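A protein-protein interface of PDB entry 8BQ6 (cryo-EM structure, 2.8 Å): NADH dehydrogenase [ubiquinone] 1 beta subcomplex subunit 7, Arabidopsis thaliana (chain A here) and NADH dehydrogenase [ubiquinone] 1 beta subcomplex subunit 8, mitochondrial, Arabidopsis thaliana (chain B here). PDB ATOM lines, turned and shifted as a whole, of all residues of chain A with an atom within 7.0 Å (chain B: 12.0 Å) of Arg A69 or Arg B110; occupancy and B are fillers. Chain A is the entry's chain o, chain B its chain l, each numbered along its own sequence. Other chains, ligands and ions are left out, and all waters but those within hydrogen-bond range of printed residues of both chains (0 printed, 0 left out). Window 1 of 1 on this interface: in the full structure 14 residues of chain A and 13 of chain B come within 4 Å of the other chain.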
ATOM      1  N   GLY A  25      32.237   8.880  22.662  1.00  0.00           N
ATOM      2  CA  GLY A  25      30.835   9.168  22.448  1.00  0.00           C
ATOM      3  C   GLY A  25      30.063   8.062  21.761  1.00  0.00           C
ATOM      4  O   GLY A  25      28.829   8.111  21.755  1.00  0.00           O
ATOM      5  N   SER A  26      30.752   7.076  21.183  1.00  0.00           N
ATOM      6  CA  SER A  26      30.117   5.924  20.554  1.00  0.00           C
ATOM      7  C   SER A  26      30.351   4.638  21.342  1.00  0.00           C
ATOM      8  O   SER A  26      30.285   3.541  20.782  1.00  0.00           O
ATOM      9  CB  SER A  26      30.604   5.753  19.115  1.00  0.00           C
ATOM     10  OG  SER A  26      30.124   6.788  18.279  1.00  0.00           O
ATOM     11  N   ARG A  27      30.653   4.758  22.630  1.00  0.00           N
ATOM     12  CA  ARG A  27      30.747   3.602  23.522  1.00  0.00           C
ATOM     13  C   ARG A  27      29.436   3.416  24.284  1.00  0.00           C
ATOM     14  O   ARG A  27      29.386   3.439  25.512  1.00  0.00           O
ATOM     15  CB  ARG A  27      31.926   3.766  24.475  1.00  0.00           C
ATOM     16  CG  ARG A  27      33.243   3.960  23.767  1.00  0.00           C
ATOM     17  CD  ARG A  27      34.423   3.934  24.717  1.00  0.00           C
ATOM     18  NE  ARG A  27      35.670   3.838  23.970  1.00  0.00           N
ATOM     19  CZ  ARG A  27      36.853   3.567  24.502  1.00  0.00           C
ATOM     20  NH1 ARG A  27      36.999   3.368  25.800  1.00  0.00           N
ATOM     21  NH2 ARG A  27      37.919   3.501  23.710  1.00  0.00           N
ATOM     22  N   ASP A  28      28.359   3.245  23.524  1.00  0.00           N
ATOM     23  CA  ASP A  28      27.022   3.057  24.063  1.00  0.00           C
ATOM     24  C   ASP A  28      26.589   1.599  23.880  1.00  0.00           C
ATOM     25  O   ASP A  28      27.403   0.734  23.539  1.00  0.00           O
ATOM     26  CB  ASP A  28      26.056   4.059  23.417  1.00  0.00           C
ATOM     27  CG  ASP A  28      26.126   4.052  21.906  1.00  0.00           C
ATOM     28  OD1 ASP A  28      26.979   3.335  21.347  1.00  0.00           O
ATOM     29  OD2 ASP A  28      25.326   4.773  21.276  1.00  0.00           O
ATOM     30  N   GLU A  62      20.954   1.916  16.905  1.00  0.00           N
ATOM     31  CA  GLU A  62      21.001   3.293  17.388  1.00  0.00           C
ATOM     32  C   GLU A  62      19.638   3.962  17.279  1.00  0.00           C
ATOM     33  O   GLU A  62      19.281   4.794  18.118  1.00  0.00           O
ATOM     34  CB  GLU A  62      22.057   4.091  16.626  1.00  0.00           C
ATOM     35  CG  GLU A  62      23.479   3.648  16.903  1.00  0.00           C
ATOM     36  CD  GLU A  62      24.014   4.169  18.225  1.00  0.00           C
ATOM     37  OE1 GLU A  62      23.284   4.891  18.933  1.00  0.00           O
ATOM     38  OE2 GLU A  62      25.169   3.847  18.561  1.00  0.00           O
ATOM     39  N   GLU A  64      16.886   2.265  17.670  1.00  0.00           N
ATOM     40  CA  GLU A  64      16.163   1.661  18.781  1.00  0.00           C
ATOM     41  C   GLU A  64      16.477   2.374  20.090  1.00  0.00           C
ATOM     42  O   GLU A  64      15.592   2.560  20.931  1.00  0.00           O
ATOM     43  CB  GLU A  64      16.513   0.177  18.872  1.00  0.00           C
ATOM     44  CG  GLU A  64      15.546  -0.733  18.134  1.00  0.00           C
ATOM     45  CD  GLU A  64      15.330  -2.047  18.850  1.00  0.00           C
ATOM     46  OE1 GLU A  64      16.105  -2.992  18.598  1.00  0.00           O
ATOM     47  OE2 GLU A  64      14.393  -2.132  19.672  1.00  0.00           O
ATOM     48  N   LEU A  65      17.733   2.786  20.278  1.00  0.00           N
ATOM     49  CA  LEU A  65      18.110   3.437  21.528  1.00  0.00           C
ATOM     50  C   LEU A  65      17.429   4.793  21.671  1.00  0.00           C
ATOM     51  O   LEU A  65      16.913   5.130  22.743  1.00  0.00           O
ATOM     52  CB  LEU A  65      19.628   3.585  21.607  1.00  0.00           C
ATOM     53  CG  LEU A  65      20.359   2.619  22.541  1.00  0.00           C
ATOM     54  CD1 LEU A  65      19.922   2.787  23.985  1.00  0.00           C
ATOM     55  CD2 LEU A  65      20.136   1.195  22.077  1.00  0.00           C
ATOM     56  N   VAL A  66      17.418   5.586  20.597  1.00  0.00           N
ATOM     57  CA  VAL A  66      16.871   6.939  20.681  1.00  0.00           C
ATOM     58  C   VAL A  66      15.363   6.895  20.880  1.00  0.00           C
ATOM     59  O   VAL A  66      14.790   7.726  21.596  1.00  0.00           O
ATOM     60  CB  VAL A  66      17.255   7.754  19.433  1.00  0.00           C
ATOM     61  CG1 VAL A  66      16.826   9.202  19.596  1.00  0.00           C
ATOM     62  CG2 VAL A  66      18.749   7.674  19.187  1.00  0.00           C
ATOM     63  N   MET A  67      14.707   5.930  20.236  1.00  0.00           N
ATOM     64  CA  MET A  67      13.242   5.764  20.433  1.00  0.00           C
ATOM     65  C   MET A  67      12.973   5.432  21.903  1.00  0.00           C
ATOM     66  O   MET A  67      12.012   5.978  22.455  1.00  0.00           O
ATOM     67  CB  MET A  67      12.705   4.640  19.546  1.00  0.00           C
ATOM     68  CG  MET A  67      12.840   4.931  18.068  1.00  0.00           C
ATOM     69  SD  MET A  67      11.879   6.373  17.549  1.00  0.00           S
ATOM     70  CE  MET A  67      13.173   7.602  17.404  1.00  0.00           C
ATOM     71  N   GLU A  68      13.796   4.575  22.503  1.00  0.00           N
ATOM     72  CA  GLU A  68      13.611   4.164  23.918  1.00  0.00           C
ATOM     73  C   GLU A  68      13.641   5.394  24.836  1.00  0.00           C
ATOM     74  O   GLU A  68      12.722   5.518  25.665  1.00  0.00           O
ATOM     75  CB  GLU A  68      14.699   3.158  24.278  1.00  0.00           C
ATOM     76  CG  GLU A  68      14.337   2.223  25.415  1.00  0.00           C
ATOM     77  CD  GLU A  68      15.533   1.533  26.051  1.00  0.00           C
ATOM     78  OE1 GLU A  68      16.588   1.447  25.394  1.00  0.00           O
ATOM     79  OE2 GLU A  68      15.409   1.085  27.206  1.00  0.00           O
ATOM     80  N   ARG A  69      14.644   6.271  24.681  1.00  0.00           N
ATOM     81  CA  ARG A  69      14.753   7.508  25.502  1.00  0.00           C
ATOM     82  C   ARG A  69      13.635   8.485  25.134  1.00  0.00           C
ATOM     83  O   ARG A  69      13.167   9.195  26.043  1.00  0.00           O
ATOM     84  CB  ARG A  69      16.115   8.171  25.300  1.00  0.00           C
ATOM     85  CG  ARG A  69      17.299   7.318  25.731  1.00  0.00           C
ATOM     86  CD  ARG A  69      18.583   7.759  25.060  1.00  0.00           C
ATOM     87  NE  ARG A  69      18.629   9.203  24.874  1.00  0.00           N
ATOM     88  CZ  ARG A  69      19.062   9.812  23.779  1.00  0.00           C
ATOM     89  NH1 ARG A  69      19.508   9.106  22.754  1.00  0.00           N
ATOM     90  NH2 ARG A  69      19.055  11.130  23.718  1.00  0.00           N
ATOM     91  N   MET A  70      13.230   8.527  23.864  1.00  0.00           N
ATOM     92  CA  MET A  70      12.089   9.382  23.449  1.00  0.00           C
ATOM     93  C   MET A  70      10.823   8.929  24.185  1.00  0.00           C
ATOM     94  O   MET A  70      10.078   9.813  24.643  1.00  0.00           O
ATOM     95  CB  MET A  70      11.847   9.274  21.941  1.00  0.00           C
ATOM     96  CG  MET A  70      12.555  10.330  21.123  1.00  0.00           C
ATOM     97  SD  MET A  70      11.728  10.607  19.540  1.00  0.00           S
ATOM     98  CE  MET A  70      10.565  11.893  19.991  1.00  0.00           C
ATOM     99  N   LEU A  71      10.598   7.614  24.296  1.00  0.00           N
ATOM    100  CA  LEU A  71       9.385   7.063  24.965  1.00  0.00           C
ATOM    101  C   LEU A  71       9.461   7.308  26.472  1.00  0.00           C
ATOM    102  O   LEU A  71       8.400   7.515  27.083  1.00  0.00           O
ATOM    103  CB  LEU A  71       9.295   5.562  24.673  1.00  0.00           C
ATOM    104  CG  LEU A  71       8.566   5.200  23.382  1.00  0.00           C
ATOM    105  CD1 LEU A  71       9.076   3.885  22.819  1.00  0.00           C
ATOM    106  CD2 LEU A  71       7.064   5.137  23.614  1.00  0.00           C
ATOM    107  N   ALA A  72      10.663   7.262  27.048  1.00  0.00           N
ATOM    108  CA  ALA A  72      10.833   7.528  28.495  1.00  0.00           C
ATOM    109  C   ALA A  72      10.417   8.966  28.804  1.00  0.00           C
ATOM    110  O   ALA A  72       9.804   9.185  29.855  1.00  0.00           O
ATOM    111  CB  ALA A  72      12.262   7.275  28.887  1.00  0.00           C
ATOM    112  N   MET A  73      10.763   9.912  27.926  1.00  0.00           N
ATOM    113  CA  MET A  73      10.345  11.323  28.114  1.00  0.00           C
ATOM    114  C   MET A  73       8.852  11.425  27.811  1.00  0.00           C
ATOM    115  O   MET A  73       8.165  12.115  28.571  1.00  0.00           O
ATOM    116  CB  MET A  73      11.108  12.255  27.175  1.00  0.00           C
ATOM    117  CG  MET A  73      10.775  13.720  27.370  1.00  0.00           C
ATOM    118  SD  MET A  73      11.308  14.340  28.981  1.00  0.00           S
ATOM    119  CE  MET A  73      13.075  14.477  28.728  1.00  0.00           C
ATOM    120  N   LYS A  74       8.373  10.762  26.752  1.00  0.00           N
ATOM    121  CA  LYS A  74       6.917  10.747  26.448  1.00  0.00           C
ATOM    122  C   LYS A  74       6.177  10.442  27.747  1.00  0.00           C
ATOM    123  O   LYS A  74       5.186  11.141  28.024  1.00  0.00           O
ATOM    124  CB  LYS A  74       6.577   9.680  25.407  1.00  0.00           C
ATOM    125  CG  LYS A  74       7.130   9.921  24.012  1.00  0.00           C
ATOM    126  CD  LYS A  74       6.773   8.813  23.047  1.00  0.00           C
ATOM    127  CE  LYS A  74       7.298   9.055  21.648  1.00  0.00           C
ATOM    128  NZ  LYS A  74       6.953   7.943  20.734  1.00  0.00           N
ATOM    129  N   LYS A  75       6.663   9.463  28.514  1.00  0.00           N
ATOM    130  CA  LYS A  75       6.054   9.183  29.834  1.00  0.00           C
ATOM    131  C   LYS A  75       6.221  10.411  30.721  1.00  0.00           C
ATOM    132  O   LYS A  75       5.242  11.019  30.964  1.00  0.00           O
ATOM    133  CB  LYS A  75       6.696   7.956  30.485  1.00  0.00           C
ATOM    134  CG  LYS A  75       5.942   6.651  30.289  1.00  0.00           C
ATOM    135  CD  LYS A  75       6.328   5.588  31.293  1.00  0.00           C
ATOM    136  CE  LYS A  75       5.740   5.829  32.667  1.00  0.00           C
ATOM    137  NZ  LYS A  75       4.268   5.654  32.680  1.00  0.00           N
ATOM    138  N   ILE A  76       7.428  10.825  31.069  1.00  0.00           N
ATOM    139  CA  ILE A  76       7.693  11.888  32.041  1.00  0.00           C
ATOM    140  C   ILE A  76       6.846  13.119  31.739  1.00  0.00           C
ATOM    141  O   ILE A  76       6.345  13.794  32.647  1.00  0.00           O
ATOM    142  CB  ILE A  76       9.193  12.220  32.049  1.00  0.00           C
ATOM    143  CG1 ILE A  76       9.949  11.157  32.844  1.00  0.00           C
ATOM    144  CG2 ILE A  76       9.445  13.611  32.612  1.00  0.00           C
ATOM    145  CD1 ILE A  76      11.393  11.016  32.446  1.00  0.00           C
ATOM    146  N   ALA B 102      14.860  24.270  25.811  1.00  0.00           N
ATOM    147  CA  ALA B 102      15.450  23.262  26.684  1.00  0.00           C
ATOM    148  C   ALA B 102      14.406  22.546  27.525  1.00  0.00           C
ATOM    149  O   ALA B 102      14.638  21.410  27.951  1.00  0.00           O
ATOM    150  CB  ALA B 102      16.492  23.905  27.598  1.00  0.00           C
ATOM    151  N   LYS B 104      11.391  21.633  26.505  1.00  0.00           N
ATOM    152  CA  LYS B 104      10.543  20.770  25.689  1.00  0.00           C
ATOM    153  C   LYS B 104      11.354  19.717  24.944  1.00  0.00           C
ATOM    154  O   LYS B 104      11.050  19.393  23.795  1.00  0.00           O
ATOM    155  CB  LYS B 104       9.719  21.588  24.697  1.00  0.00           C
ATOM    156  CG  LYS B 104      10.527  22.369  23.691  1.00  0.00           C
ATOM    157  CD  LYS B 104       9.608  23.137  22.765  1.00  0.00           C
ATOM    158  CE  LYS B 104       8.887  24.241  23.507  1.00  0.00           C
ATOM    159  NZ  LYS B 104       7.980  25.002  22.602  1.00  0.00           N
ATOM    160  N   VAL B 105      12.361  19.165  25.626  1.00  0.00           N
ATOM    161  CA  VAL B 105      13.236  18.131  24.998  1.00  0.00           C
ATOM    162  C   VAL B 105      12.428  16.833  24.882  1.00  0.00           C
ATOM    163  O   VAL B 105      11.826  16.424  25.889  1.00  0.00           O
ATOM    164  CB  VAL B 105      14.561  17.971  25.777  1.00  0.00           C
ATOM    165  CG1 VAL B 105      14.383  17.916  27.286  1.00  0.00           C
ATOM    166  CG2 VAL B 105      15.432  16.835  25.275  1.00  0.00           C
ATOM    167  N   PRO B 106      12.356  16.185  23.699  1.00  0.00           N
ATOM    168  CA  PRO B 106      11.529  14.995  23.512  1.00  0.00           C
ATOM    169  C   PRO B 106      12.245  13.667  23.806  1.00  0.00           C
ATOM    170  O   PRO B 106      11.712  12.658  23.414  1.00  0.00           O
ATOM    171  CB  PRO B 106      11.180  15.103  22.022  1.00  0.00           C
ATOM    172  CG  PRO B 106      12.428  15.672  21.396  1.00  0.00           C
ATOM    173  CD  PRO B 106      13.035  16.561  22.463  1.00  0.00           C
ATOM    174  N   PHE B 107      13.391  13.694  24.489  1.00  0.00           N
ATOM    175  CA  PHE B 107      14.086  12.438  24.890  1.00  0.00           C
ATOM    176  C   PHE B 107      14.800  12.658  26.228  1.00  0.00           C
ATOM    177  O   PHE B 107      15.006  13.819  26.621  1.00  0.00           O
ATOM    178  CB  PHE B 107      15.064  11.939  23.819  1.00  0.00           C
ATOM    179  CG  PHE B 107      15.743  13.001  22.994  1.00  0.00           C
ATOM    180  CD1 PHE B 107      16.793  13.742  23.513  1.00  0.00           C
ATOM    181  CD2 PHE B 107      15.350  13.242  21.689  1.00  0.00           C
ATOM    182  CE1 PHE B 107      17.420  14.716  22.752  1.00  0.00           C
ATOM    183  CE2 PHE B 107      15.976  14.218  20.929  1.00  0.00           C
ATOM    184  CZ  PHE B 107      17.009  14.953  21.462  1.00  0.00           C
ATOM    185  N   THR B 108      15.146  11.566  26.916  1.00  0.00           N
ATOM    186  CA  THR B 108      15.885  11.676  28.203  1.00  0.00           C
ATOM    187  C   THR B 108      17.390  11.776  27.927  1.00  0.00           C
ATOM    188  O   THR B 108      17.857  11.166  26.946  1.00  0.00           O
ATOM    189  CB  THR B 108      15.563  10.505  29.139  1.00  0.00           C
ATOM    190  OG1 THR B 108      15.890   9.284  28.475  1.00  0.00           O
ATOM    191  CG2 THR B 108      14.115  10.485  29.570  1.00  0.00           C
ATOM    192  N   PRO B 109      18.159  12.531  28.739  1.00  0.00           N
ATOM    193  CA  PRO B 109      19.610  12.628  28.571  1.00  0.00           C
ATOM    194  C   PRO B 109      20.301  11.266  28.402  1.00  0.00           C
ATOM    195  O   PRO B 109      20.031  10.390  29.196  1.00  0.00           O
ATOM    196  CB  PRO B 109      20.022  13.248  29.912  1.00  0.00           C
ATOM    197  CG  PRO B 109      18.882  14.163  30.252  1.00  0.00           C
ATOM    198  CD  PRO B 109      17.660  13.380  29.827  1.00  0.00           C
ATOM    199  N   ARG B 110      21.182  11.127  27.401  1.00  0.00           N
ATOM    200  CA  ARG B 110      21.915   9.887  27.204  1.00  0.00           C
ATOM    201  C   ARG B 110      22.532   9.423  28.513  1.00  0.00           C
ATOM    202  O   ARG B 110      23.042  10.216  29.309  1.00  0.00           O
ATOM    203  CB  ARG B 110      23.015  10.061  26.165  1.00  0.00           C
ATOM    204  CG  ARG B 110      22.547  10.038  24.733  1.00  0.00           C
ATOM    205  CD  ARG B 110      23.686  10.473  23.847  1.00  0.00           C
ATOM    206  NE  ARG B 110      23.399  10.318  22.429  1.00  0.00           N
ATOM    207  CZ  ARG B 110      24.214   9.719  21.574  1.00  0.00           C
ATOM    208  NH1 ARG B 110      25.335   9.144  21.978  1.00  0.00           N
ATOM    209  NH2 ARG B 110      23.899   9.695  20.283  1.00  0.00           N
ATOM    210  N   VAL B 111      22.473   8.117  28.737  1.00  0.00           N
ATOM    211  CA  VAL B 111      23.163   7.502  29.856  1.00  0.00           C
ATOM    212  C   VAL B 111      24.149   6.514  29.252  1.00  0.00           C
ATOM    213  O   VAL B 111      23.772   5.691  28.409  1.00  0.00           O
ATOM    214  CB  VAL B 111      22.209   6.815  30.844  1.00  0.00           C
ATOM    215  CG1 VAL B 111      21.224   5.909  30.116  1.00  0.00           C
ATOM    216  CG2 VAL B 111      22.992   6.045  31.890  1.00  0.00           C
ATOM    217  N   TYR B 112      25.410   6.635  29.626  1.00  0.00           N
ATOM    218  CA  TYR B 112      26.439   5.762  29.106  1.00  0.00           C
ATOM    219  C   TYR B 112      26.770   4.686  30.131  1.00  0.00           C
ATOM    220  O   TYR B 112      26.737   4.930  31.338  1.00  0.00           O
ATOM    221  CB  TYR B 112      27.683   6.571  28.742  1.00  0.00           C
ATOM    222  CG  TYR B 112      27.549   7.317  27.431  1.00  0.00           C
ATOM    223  CD1 TYR B 112      26.892   8.538  27.363  1.00  0.00           C
ATOM    224  CD2 TYR B 112      28.067   6.790  26.257  1.00  0.00           C
ATOM    225  CE1 TYR B 112      26.759   9.212  26.163  1.00  0.00           C
ATOM    226  CE2 TYR B 112      27.940   7.458  25.056  1.00  0.00           C
ATOM    227  CZ  TYR B 112      27.288   8.667  25.015  1.00  0.00           C
ATOM    228  OH  TYR B 112      27.164   9.330  23.818  1.00  0.00           O
ATOM    229  N   PRO B 113      27.078   3.481  29.674  1.00  0.00           N
ATOM    230  CA  PRO B 113      27.347   2.383  30.610  1.00  0.00           C
ATOM    231  C   PRO B 113      28.613   2.604  31.420  1.00  0.00           C
ATOM    232  O   PRO B 113      29.378   3.534  31.147  1.00  0.00           O
ATOM    233  CB  PRO B 113      27.479   1.167  29.688  1.00  0.00           C
ATOM    234  CG  PRO B 113      27.904   1.743  28.379  1.00  0.00           C
ATOM    235  CD  PRO B 113      27.174   3.046  28.271  1.00  0.00           C
ATOM    236  N   TYR B 114      28.834   1.752  32.422  1.00  0.00           N
ATOM    237  CA  TYR B 114      30.035   1.793  33.256  1.00  0.00           C
ATOM    238  C   TYR B 114      30.151   3.129  33.990  1.00  0.00           C
ATOM    239  O   TYR B 114      31.186   3.801  33.963  1.00  0.00           O
ATOM    240  CB  TYR B 114      31.287   1.502  32.423  1.00  0.00           C
ATOM    241  CG  TYR B 114      31.255   0.153  31.744  1.00  0.00           C
ATOM    242  CD1 TYR B 114      31.406  -1.014  32.478  1.00  0.00           C
ATOM    243  CD2 TYR B 114      31.058   0.046  30.377  1.00  0.00           C
ATOM    244  CE1 TYR B 114      31.371  -2.248  31.869  1.00  0.00           C
ATOM    245  CE2 TYR B 114      31.022  -1.188  29.758  1.00  0.00           C
ATOM    246  CZ  TYR B 114      31.180  -2.330  30.510  1.00  0.00           C
ATOM    247  OH  TYR B 114      31.148  -3.563  29.905  1.00  0.00           O
ATOM    248  N   ASP B 115      29.060   3.494  34.667  1.00  0.00           N
ATOM    249  CA  ASP B 115      28.976   4.735  35.438  1.00  0.00           C
ATOM    250  C   ASP B 115      29.241   5.945  34.542  1.00  0.00           C
ATOM    251  O   ASP B 115      30.033   6.832  34.867  1.00  0.00           O
ATOM    252  CB  ASP B 115      29.933   4.700  36.635  1.00  0.00           C
ATOM    253  CG  ASP B 115      29.693   5.837  37.612  1.00  0.00           C
ATOM    254  OD1 ASP B 115      28.521   6.220  37.806  1.00  0.00           O
ATOM    255  OD2 ASP B 115      30.679   6.339  38.193  1.00  0.00           O
ATOM    256  N   ASN B 116      28.558   5.969  33.396  1.00  0.00           N
ATOM    257  CA  ASN B 116      28.702   7.042  32.412  1.00  0.00           C
ATOM    258  C   ASN B 116      30.151   7.174  31.951  1.00  0.00           C
ATOM    259  O   ASN B 116      30.669   8.280  31.786  1.00  0.00           O
ATOM    260  CB  ASN B 116      28.179   8.371  32.961  1.00  0.00           C
ATOM    261  CG  ASN B 116      26.934   8.846  32.243  1.00  0.00           C
ATOM    262  OD1 ASN B 116      26.815   8.712  31.026  1.00  0.00           O
ATOM    263  ND2 ASN B 116      25.998   9.408  32.995  1.00  0.00           N
ATOM    264  N   LEU B 117      30.806   6.030  31.753  1.00  0.00           N
ATOM    265  CA  LEU B 117      32.193   5.967  31.296  1.00  0.00           C
ATOM    266  C   LEU B 117      33.105   6.812  32.186  1.00  0.00           C
ATOM    267  O   LEU B 117      33.904   7.625  31.711  1.00  0.00           O
ATOM    268  CB  LEU B 117      32.305   6.396  29.832  1.00  0.00           C
ATOM    269  CG  LEU B 117      31.509   5.624  28.777  1.00  0.00           C
ATOM    270  CD1 LEU B 117      31.441   6.439  27.501  1.00  0.00           C
ATOM    271  CD2 LEU B 117      32.099   4.245  28.505  1.00  0.00           C
ATOM    272  N   ARG B 118      32.969   6.619  33.500  1.00  0.00           N
ATOM    273  CA  ARG B 118      33.739   7.403  34.462  1.00  0.00           C
ATOM    274  C   ARG B 118      35.235   7.137  34.325  1.00  0.00           C
ATOM    275  O   ARG B 118      36.048   8.069  34.362  1.00  0.00           O
ATOM    276  CB  ARG B 118      33.265   7.090  35.881  1.00  0.00           C
ATOM    277  CG  ARG B 118      34.045   7.792  36.980  1.00  0.00           C
ATOM    278  CD  ARG B 118      33.818   7.124  38.331  1.00  0.00           C
ATOM    279  NE  ARG B 118      34.761   6.037  38.568  1.00  0.00           N
ATOM    280  CZ  ARG B 118      34.470   4.748  38.450  1.00  0.00           C
ATOM    281  NH1 ARG B 118      33.255   4.340  38.124  1.00  0.00           N
ATOM    282  NH2 ARG B 118      35.424   3.847  38.664  1.00  0.00           N
ATOM    283  N   LEU B 121      36.816   8.415  30.994  1.00  0.00           N
ATOM    284  CA  LEU B 121      36.909   9.864  30.894  1.00  0.00           C
ATOM    285  C   LEU B 121      37.967  10.454  31.816  1.00  0.00           C
ATOM    286  O   LEU B 121      37.991  11.674  32.012  1.00  0.00           O
ATOM    287  CB  LEU B 121      35.550  10.496  31.191  1.00  0.00           C
ATOM    288  CG  LEU B 121      34.635  10.676  29.983  1.00  0.00           C
ATOM    289  CD1 LEU B 121      33.362  11.395  30.390  1.00  0.00           C
ATOM    290  CD2 LEU B 121      35.358  11.442  28.896  1.00  0.00           C
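The backbone carbonyl oxygen of Thr B108 lies within hydrogen-bond range of the guanidinium group of Arg A69, 3.0 Å away. The backbone carbonyl oxygen (O) of Gly A25 is in hydrogen-bond range of the side-chain hydroxyl (OH) of Tyr B112 (2.9 Å). SD of Met A73 lies close to O of Val B105 (3.8 Å).
The side-chain hydroxyl (OH) of Tyr B112 lies within hydrogen-bond range of the guanidinium group (NH1) of Arg B110 (2.6 Å). N of Tyr B112 lies within hydrogen-bond range of OD1 of Asn B116 (2.9 Å).
NH1 of Arg B110 touches O of Gly A25, at 3.7 Å. Tyr B112 touches Arg A27. Arg A27 touches Pro B113 (O to CD, 3.6 Å). Phe B107 touches Arg A69 (CD1 to NH2, 3.5 Å). CG of Arg B110 touches CZ of Arg A69, 3.6 Å away. Met A70 touches Phe B107 (N to CB, 3.9 Å). Thr B108 touches Ala A72. Met A73 touches Pro B106. Phe B107 touches Met A73 (O to CE, 2.9 Å). N of Met A73 touches CG2 of Thr B108 (3.8 Å).
Of chain B, only Phe B107 (3.5 Å), Thr B108 (3.0 Å) and Arg B110 (3.6 Å) come within 4 Å of Arg A69. Printed residues of chain A within 4 Å of Arg B110: Gly A25 (3.7 Å) and Arg A69 (3.6 Å). No residue of chain B comes within 4 Å of Ser A26. No residue of chain B comes within 4 Å of Val A66. No residue of chain B comes within 4 Å of Met A67. Of chain B, only Pro B106 (3.3 Å) and Phe B107 (3.9 Å) come within 4 Å of Met A70. Of chain B, only Val B105, Pro B106, Phe B107 and Thr B108 come within 4 Å of Met A73. Printed residues of chain B within 4 Å of Ile A76: Thr B108 (3.995 Å). Printed residues of chain B within 4 Å of Arg A27: Tyr B112 (3.7 Å) and Pro B113 (3.6 Å). Printed residues of chain A within 4 Å of Tyr B112: Gly A25 and Arg A27. Of the printed residues of chain A, Pro B113 touches Arg A27 (3.6 Å). Of the printed residues of chain A, Phe B107 touches Arg A69, Met A70 and Met A73. Leu B121 touches none of the printed residues of chain A. Asn B116 touches none of the printed residues of chain A. The nearest residue of chain A that does not touch Arg B110 is Asp A28 (4.4 Å). The nearest printed residue of chain A that does not touch Phe B107 is Val A66 (4.8 Å).
Of the 18 printed residues of chain A, 7 touch a printed residue of chain B. Printed residues of chain A that touch a printed residue of chain B: Gly A25, Arg A27, Arg A69, Met A70, Ala A72, Met A73 and Ile A76. Hydrophobic or aromatic side chains of chain B within 4 Å of the printed part of chain A: Val B105, Pro B106, Phe B107, Tyr B112 and Pro B113. Among the printed residues, no Asp or Glu carboxylate lies within 4 Å of a Lys or Arg side-chain nitrogen of the other chain.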
